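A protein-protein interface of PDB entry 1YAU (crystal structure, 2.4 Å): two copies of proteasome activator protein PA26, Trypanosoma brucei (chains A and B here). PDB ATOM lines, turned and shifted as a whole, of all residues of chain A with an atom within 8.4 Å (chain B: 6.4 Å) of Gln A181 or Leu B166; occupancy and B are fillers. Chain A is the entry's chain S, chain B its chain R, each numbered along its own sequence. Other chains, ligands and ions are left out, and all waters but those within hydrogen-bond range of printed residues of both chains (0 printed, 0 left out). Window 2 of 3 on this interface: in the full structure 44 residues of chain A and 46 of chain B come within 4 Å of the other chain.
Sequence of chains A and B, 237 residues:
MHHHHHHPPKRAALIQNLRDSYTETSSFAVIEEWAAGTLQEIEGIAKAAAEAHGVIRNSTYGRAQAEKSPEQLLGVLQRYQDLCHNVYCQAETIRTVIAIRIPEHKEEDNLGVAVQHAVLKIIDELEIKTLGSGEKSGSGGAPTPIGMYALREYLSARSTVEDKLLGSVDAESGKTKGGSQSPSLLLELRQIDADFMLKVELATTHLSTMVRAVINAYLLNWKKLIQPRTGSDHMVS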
ATOM      1  N   ARG A  63     -15.369  36.292  16.958  1.00  0.00           N
ATOM      2  CA  ARG A  63     -15.156  36.664  18.347  1.00  0.00           C
ATOM      3  C   ARG A  63     -14.661  38.126  18.524  1.00  0.00           C
ATOM      4  O   ARG A  63     -14.932  38.750  19.544  1.00  0.00           O
ATOM      5  CB  ARG A  63     -14.251  35.609  19.020  1.00  0.00           C
ATOM      6  CG  ARG A  63     -14.004  35.730  20.530  1.00  0.00           C
ATOM      7  CD  ARG A  63     -12.730  35.006  20.988  1.00  0.00           C
ATOM      8  NE  ARG A  63     -12.322  35.421  22.331  1.00  0.00           N
ATOM      9  CZ  ARG A  63     -12.760  34.839  23.451  1.00  0.00           C
ATOM     10  NH1 ARG A  63     -13.615  33.813  23.375  1.00  0.00           N
ATOM     11  NH2 ARG A  63     -12.351  35.279  24.645  1.00  0.00           N
ATOM     12  N   LYS A 164     -21.337  35.018  27.272  1.00  0.00           N
ATOM     13  CA  LYS A 164     -21.414  33.626  26.846  1.00  0.00           C
ATOM     14  C   LYS A 164     -20.361  33.296  25.796  1.00  0.00           C
ATOM     15  O   LYS A 164     -19.878  32.164  25.757  1.00  0.00           O
ATOM     16  CB  LYS A 164     -22.788  33.297  26.276  1.00  0.00           C
ATOM     17  CG  LYS A 164     -23.839  32.983  27.320  1.00  0.00           C
ATOM     18  CD  LYS A 164     -25.204  32.834  26.666  1.00  0.00           C
ATOM     19  CE  LYS A 164     -26.325  33.212  27.623  1.00  0.00           C
ATOM     20  NZ  LYS A 164     -26.973  32.018  28.237  1.00  0.00           N
ATOM     21  N   LEU A 165     -20.010  34.281  24.961  1.00  0.00           N
ATOM     22  CA  LEU A 165     -19.090  34.063  23.841  1.00  0.00           C
ATOM     23  C   LEU A 165     -17.636  34.081  24.284  1.00  0.00           C
ATOM     24  O   LEU A 165     -16.821  33.295  23.798  1.00  0.00           O
ATOM     25  CB  LEU A 165     -19.311  35.094  22.724  1.00  0.00           C
ATOM     26  CG  LEU A 165     -20.494  34.794  21.797  1.00  0.00           C
ATOM     27  CD1 LEU A 165     -20.759  35.941  20.823  1.00  0.00           C
ATOM     28  CD2 LEU A 165     -20.273  33.442  21.076  1.00  0.00           C
ATOM     29  N   GLY A 178     -13.541  29.297  29.031  1.00  0.00           N
ATOM     30  CA  GLY A 178     -13.691  29.160  27.546  1.00  0.00           C
ATOM     31  C   GLY A 178     -15.098  29.523  27.078  1.00  0.00           C
ATOM     32  O   GLY A 178     -16.096  29.127  27.712  1.00  0.00           O
ATOM     33  N   GLY A 179     -15.179  30.275  25.970  1.00  0.00           N
ATOM     34  CA  GLY A 179     -16.461  30.720  25.409  1.00  0.00           C
ATOM     35  C   GLY A 179     -17.325  29.591  24.889  1.00  0.00           C
ATOM     36  O   GLY A 179     -16.897  28.444  24.862  1.00  0.00           O
ATOM     37  N   SER A 180     -18.549  29.921  24.482  1.00  0.00           N
ATOM     38  CA  SER A 180     -19.474  28.945  23.909  1.00  0.00           C
ATOM     39  C   SER A 180     -19.085  28.554  22.473  1.00  0.00           C
ATOM     40  O   SER A 180     -18.629  29.383  21.682  1.00  0.00           O
ATOM     41  CB  SER A 180     -20.904  29.493  23.945  1.00  0.00           C
ATOM     42  OG  SER A 180     -21.806  28.655  23.237  1.00  0.00           O
ATOM     43  N   GLN A 181     -19.274  27.282  22.147  1.00  0.00           N
ATOM     44  CA  GLN A 181     -19.002  26.782  20.796  1.00  0.00           C
ATOM     45  C   GLN A 181     -20.246  26.817  19.887  1.00  0.00           C
ATOM     46  O   GLN A 181     -20.136  26.566  18.675  1.00  0.00           O
ATOM     47  CB  GLN A 181     -18.407  25.365  20.848  1.00  0.00           C
ATOM     48  CG  GLN A 181     -17.143  25.246  21.721  1.00  0.00           C
ATOM     49  CD  GLN A 181     -15.858  25.683  21.008  1.00  0.00           C
ATOM     50  OE1 GLN A 181     -15.779  26.791  20.460  1.00  0.00           O
ATOM     51  NE2 GLN A 181     -14.842  24.809  21.033  1.00  0.00           N
ATOM     52  N   SER A 182     -21.411  27.147  20.472  1.00  0.00           N
ATOM     53  CA  SER A 182     -22.672  27.298  19.715  1.00  0.00           C
ATOM     54  C   SER A 182     -22.543  28.234  18.495  1.00  0.00           C
ATOM     55  O   SER A 182     -22.236  29.409  18.656  1.00  0.00           O
ATOM     56  CB  SER A 182     -23.795  27.766  20.638  1.00  0.00           C
ATOM     57  OG  SER A 182     -24.996  27.986  19.908  1.00  0.00           O
ATOM     58  N   PRO A 183     -22.731  27.699  17.282  1.00  0.00           N
ATOM     59  CA  PRO A 183     -22.647  28.507  16.054  1.00  0.00           C
ATOM     60  C   PRO A 183     -23.797  29.536  15.922  1.00  0.00           C
ATOM     61  O   PRO A 183     -23.549  30.671  15.498  1.00  0.00           O
ATOM     62  CB  PRO A 183     -22.715  27.466  14.940  1.00  0.00           C
ATOM     63  CG  PRO A 183     -23.413  26.318  15.529  1.00  0.00           C
ATOM     64  CD  PRO A 183     -23.038  26.284  16.990  1.00  0.00           C
ATOM     65  N   SER A 184     -25.022  29.153  16.295  1.00  0.00           N
ATOM     66  CA  SER A 184     -26.174  30.090  16.333  1.00  0.00           C
ATOM     67  C   SER A 184     -25.991  31.297  17.273  1.00  0.00           C
ATOM     68  O   SER A 184     -26.451  32.393  16.952  1.00  0.00           O
ATOM     69  CB  SER A 184     -27.478  29.365  16.697  1.00  0.00           C
ATOM     70  OG  SER A 184     -27.876  28.488  15.667  1.00  0.00           O
ATOM     71  N   LEU A 185     -25.318  31.098  18.409  1.00  0.00           N
ATOM     72  CA  LEU A 185     -25.076  32.170  19.375  1.00  0.00           C
ATOM     73  C   LEU A 185     -24.218  33.303  18.821  1.00  0.00           C
ATOM     74  O   LEU A 185     -24.437  34.463  19.165  1.00  0.00           O
ATOM     75  CB  LEU A 185     -24.479  31.610  20.672  1.00  0.00           C
ATOM     76  CG  LEU A 185     -24.165  32.584  21.815  1.00  0.00           C
ATOM     77  CD1 LEU A 185     -25.424  33.096  22.522  1.00  0.00           C
ATOM     78  CD2 LEU A 185     -23.260  31.920  22.819  1.00  0.00           C
ATOM     79  N   LEU A 186     -23.253  32.981  17.958  1.00  0.00           N
ATOM     80  CA  LEU A 186     -22.438  34.005  17.287  1.00  0.00           C
ATOM     81  C   LEU A 186     -23.237  34.717  16.204  1.00  0.00           C
ATOM     82  O   LEU A 186     -23.041  35.914  15.952  1.00  0.00           O
ATOM     83  CB  LEU A 186     -21.156  33.383  16.688  1.00  0.00           C
ATOM     84  CG  LEU A 186     -20.169  34.243  15.868  1.00  0.00           C
ATOM     85  CD1 LEU A 186     -19.774  35.521  16.591  1.00  0.00           C
ATOM     86  CD2 LEU A 186     -18.896  33.455  15.520  1.00  0.00           C
ATOM     87  N   ARG B  63     -24.456  15.394  16.402  1.00  0.00           N
ATOM     88  CA  ARG B  63     -23.938  16.681  16.893  1.00  0.00           C
ATOM     89  C   ARG B  63     -23.179  17.490  15.827  1.00  0.00           C
ATOM     90  O   ARG B  63     -22.730  18.608  16.095  1.00  0.00           O
ATOM     91  CB  ARG B  63     -23.190  16.570  18.252  1.00  0.00           C
ATOM     92  CG  ARG B  63     -21.905  15.729  18.266  1.00  0.00           C
ATOM     93  CD  ARG B  63     -21.082  15.840  19.574  1.00  0.00           C
ATOM     94  NE  ARG B  63     -20.138  16.959  19.503  1.00  0.00           N
ATOM     95  CZ  ARG B  63     -19.710  17.661  20.546  1.00  0.00           C
ATOM     96  NH1 ARG B  63     -20.141  17.369  21.774  1.00  0.00           N
ATOM     97  NH2 ARG B  63     -18.850  18.661  20.356  1.00  0.00           N
ATOM     98  N   ALA B  66     -25.519  20.223  15.272  1.00  0.00           N
ATOM     99  CA  ALA B  66     -25.454  21.191  16.367  1.00  0.00           C
ATOM    100  C   ALA B  66     -24.220  22.073  16.274  1.00  0.00           C
ATOM    101  O   ALA B  66     -24.005  22.945  17.120  1.00  0.00           O
ATOM    102  CB  ALA B  66     -25.468  20.469  17.692  1.00  0.00           C
ATOM    103  N   GLU B  67     -23.418  21.839  15.241  1.00  0.00           N
ATOM    104  CA  GLU B  67     -22.075  22.385  15.121  1.00  0.00           C
ATOM    105  C   GLU B  67     -22.095  23.418  14.015  1.00  0.00           C
ATOM    106  O   GLU B  67     -21.230  24.290  13.931  1.00  0.00           O
ATOM    107  CB  GLU B  67     -21.125  21.253  14.716  1.00  0.00           C
ATOM    108  CG  GLU B  67     -19.885  21.082  15.586  1.00  0.00           C
ATOM    109  CD  GLU B  67     -19.545  19.611  15.810  1.00  0.00           C
ATOM    110  OE1 GLU B  67     -19.318  18.904  14.808  1.00  0.00           O
ATOM    111  OE2 GLU B  67     -19.518  19.159  16.981  1.00  0.00           O
ATOM    112  N   VAL B 161     -30.122  24.823  22.821  1.00  0.00           N
ATOM    113  CA  VAL B 161     -29.957  23.401  22.533  1.00  0.00           C
ATOM    114  C   VAL B 161     -28.541  23.075  22.025  1.00  0.00           C
ATOM    115  O   VAL B 161     -28.014  22.016  22.334  1.00  0.00           O
ATOM    116  CB  VAL B 161     -31.043  22.929  21.515  1.00  0.00           C
ATOM    117  CG1 VAL B 161     -30.811  21.480  21.043  1.00  0.00           C
ATOM    118  CG2 VAL B 161     -32.441  23.092  22.117  1.00  0.00           C
ATOM    119  N   GLU B 162     -27.939  23.988  21.260  1.00  0.00           N
ATOM    120  CA  GLU B 162     -26.576  23.807  20.790  1.00  0.00           C
ATOM    121  C   GLU B 162     -25.615  23.763  21.955  1.00  0.00           C
ATOM    122  O   GLU B 162     -24.768  22.875  22.018  1.00  0.00           O
ATOM    123  CB  GLU B 162     -26.159  24.903  19.803  1.00  0.00           C
ATOM    124  CG  GLU B 162     -26.676  24.700  18.391  1.00  0.00           C
ATOM    125  CD  GLU B 162     -26.610  25.973  17.566  1.00  0.00           C
ATOM    126  OE1 GLU B 162     -25.945  26.918  18.031  1.00  0.00           O
ATOM    127  OE2 GLU B 162     -27.215  26.032  16.457  1.00  0.00           O
ATOM    128  N   ASP B 163     -25.747  24.705  22.882  1.00  0.00           N
ATOM    129  CA  ASP B 163     -24.901  24.718  24.057  1.00  0.00           C
ATOM    130  C   ASP B 163     -25.005  23.450  24.856  1.00  0.00           C
ATOM    131  O   ASP B 163     -23.980  22.869  25.224  1.00  0.00           O
ATOM    132  CB  ASP B 163     -25.228  25.896  24.942  1.00  0.00           C
ATOM    133  CG  ASP B 163     -24.367  27.055  24.638  1.00  0.00           C
ATOM    134  OD1 ASP B 163     -23.242  26.801  24.147  1.00  0.00           O
ATOM    135  OD2 ASP B 163     -24.720  28.247  24.829  1.00  0.00           O
ATOM    136  N   LYS B 164     -26.244  23.031  25.114  1.00  0.00           N
ATOM    137  CA  LYS B 164     -26.545  21.829  25.873  1.00  0.00           C
ATOM    138  C   LYS B 164     -25.912  20.587  25.260  1.00  0.00           C
ATOM    139  O   LYS B 164     -25.395  19.746  25.984  1.00  0.00           O
ATOM    140  CB  LYS B 164     -28.062  21.645  25.983  1.00  0.00           C
ATOM    141  CG  LYS B 164     -28.755  22.426  27.122  1.00  0.00           C
ATOM    142  CD  LYS B 164     -30.288  22.271  27.021  1.00  0.00           C
ATOM    143  CE  LYS B 164     -30.989  22.458  28.370  1.00  0.00           C
ATOM    144  NZ  LYS B 164     -30.974  23.869  28.875  1.00  0.00           N
ATOM    145  N   LEU B 165     -25.937  20.495  23.930  1.00  0.00           N
ATOM    146  CA  LEU B 165     -25.460  19.316  23.194  1.00  0.00           C
ATOM    147  C   LEU B 165     -23.945  19.249  23.066  1.00  0.00           C
ATOM    148  O   LEU B 165     -23.364  18.161  23.119  1.00  0.00           O
ATOM    149  CB  LEU B 165     -26.078  19.260  21.789  1.00  0.00           C
ATOM    150  CG  LEU B 165     -27.532  18.808  21.655  1.00  0.00           C
ATOM    151  CD1 LEU B 165     -28.054  19.118  20.273  1.00  0.00           C
ATOM    152  CD2 LEU B 165     -27.694  17.324  21.968  1.00  0.00           C
ATOM    153  N   LEU B 166     -23.319  20.411  22.870  1.00  0.00           N
ATOM    154  CA  LEU B 166     -21.867  20.530  22.717  1.00  0.00           C
ATOM    155  C   LEU B 166     -21.140  20.509  24.057  1.00  0.00           C
ATOM    156  O   LEU B 166     -20.082  19.886  24.180  1.00  0.00           O
ATOM    157  CB  LEU B 166     -21.495  21.797  21.929  1.00  0.00           C
ATOM    158  CG  LEU B 166     -22.027  21.917  20.493  1.00  0.00           C
ATOM    159  CD1 LEU B 166     -21.563  23.196  19.826  1.00  0.00           C
ATOM    160  CD2 LEU B 166     -21.638  20.715  19.667  1.00  0.00           C
ATOM    161  N   GLY B 167     -21.719  21.181  25.054  1.00  0.00           N
ATOM    162  CA  GLY B 167     -21.096  21.334  26.369  1.00  0.00           C
ATOM    163  C   GLY B 167     -19.796  22.118  26.296  1.00  0.00           C
ATOM    164  O   GLY B 167     -18.708  21.655  26.684  1.00  0.00           O
ATOM    165  N   GLY B 178     -18.018  16.371  26.758  1.00  0.00           N
ATOM    166  CA  GLY B 178     -19.361  15.879  26.313  1.00  0.00           C
ATOM    167  C   GLY B 178     -20.474  16.831  26.733  1.00  0.00           C
ATOM    168  O   GLY B 178     -20.424  17.447  27.813  1.00  0.00           O
ATOM    169  N   GLY B 179     -21.478  16.957  25.871  1.00  0.00           N
ATOM    170  CA  GLY B 179     -22.599  17.846  26.129  1.00  0.00           C
ATOM    171  C   GLY B 179     -23.676  17.151  26.922  1.00  0.00           C
ATOM    172  O   GLY B 179     -23.551  16.996  28.141  1.00  0.00           O
ATOM    173  N   SER B 180     -24.729  16.734  26.223  1.00  0.00           N
ATOM    174  CA  SER B 180     -25.853  16.040  26.839  1.00  0.00           C
ATOM    175  C   SER B 180     -26.182  14.722  26.161  1.00  0.00           C
ATOM    176  O   SER B 180     -26.180  14.620  24.926  1.00  0.00           O
ATOM    177  CB  SER B 180     -27.095  16.916  26.828  1.00  0.00           C
ATOM    178  OG  SER B 180     -28.250  16.135  27.081  1.00  0.00           O
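6 positions are printed for both chains.
The guanidinium group (NE) of Arg B63 is in salt-bridge range of the side-chain carboxylate (OE2) of Glu B67 (3.4 Å). The guanidinium group of Arg B63 lies within hydrogen-bond range of the backbone carbonyl oxygen of Leu B166 (3.5 Å). O of Lys A164 is in hydrogen-bond range of N of Ser A180. The backbone NH (N) of Ser A182 sits at hydrogen-bond distance from the side-chain hydroxyl (OG) of Ser A180 (3.2 Å). OG of Ser A182 lies within hydrogen-bond range of N of Leu A185 (3.5 Å).
Along chain A the printed residues that touch a printed residue of chain B span positions 180 to 184. Among the printed residues, 8 pairs touch across the chains. Among the printed residues, no Asp or Glu carboxylate lies within 4 Å of a Lys or Arg side-chain nitrogen of the other chain.
OE2 of Glu B162 is in hydrogen-bond range of OG of Ser A184, 2.7 Å away. The side-chain hydroxyl (OG) of Ser A180 sits at hydrogen-bond distance from the side-chain carboxylate (OD1) of Asp B163. OG of Ser A182 sits close to OE1 of Glu B162 (2.4 Å). The backbone nitrogen (N) of Pro A183 sits close to the side-chain carboxylate (OE1) of Glu B162 (3.4 Å).
Of chain B, only Leu B166 (3.8 Å) comes within 4 Å of Gln A181. Of the printed residues of chain A, Leu B166 touches Gln A181 (3.8 Å). Gly B167 touches none of the printed residues of chain A. Of the printed residues of chain B, Ser A182 touches Glu B162 and Asp B163. Printed residues of chain B within 4 Å of Ser A180: Asp B163. Printed residues of chain A within 4 Å of Asp B163: Ser A180 and Ser A182. Printed residues of chain B within 4 Å of Ser A184: Glu B162. Printed residues of chain A within 4 Å of Glu B162: Ser A182 (2.4 Å), Pro A183 (3.2 Å) and Ser A184 (2.7 Å). Lys A164 touches none of the printed residues of chain B. The nearest residue of chain B that does not touch Gln A181 is Asp B163 (4.5 Å).
Among the printed residues, pairs that only touch across the chains: Gln A181 with Leu B166, Ser A182 with Asp B163, Pro A183 with Ala B66 and Pro A183 with Glu B67.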
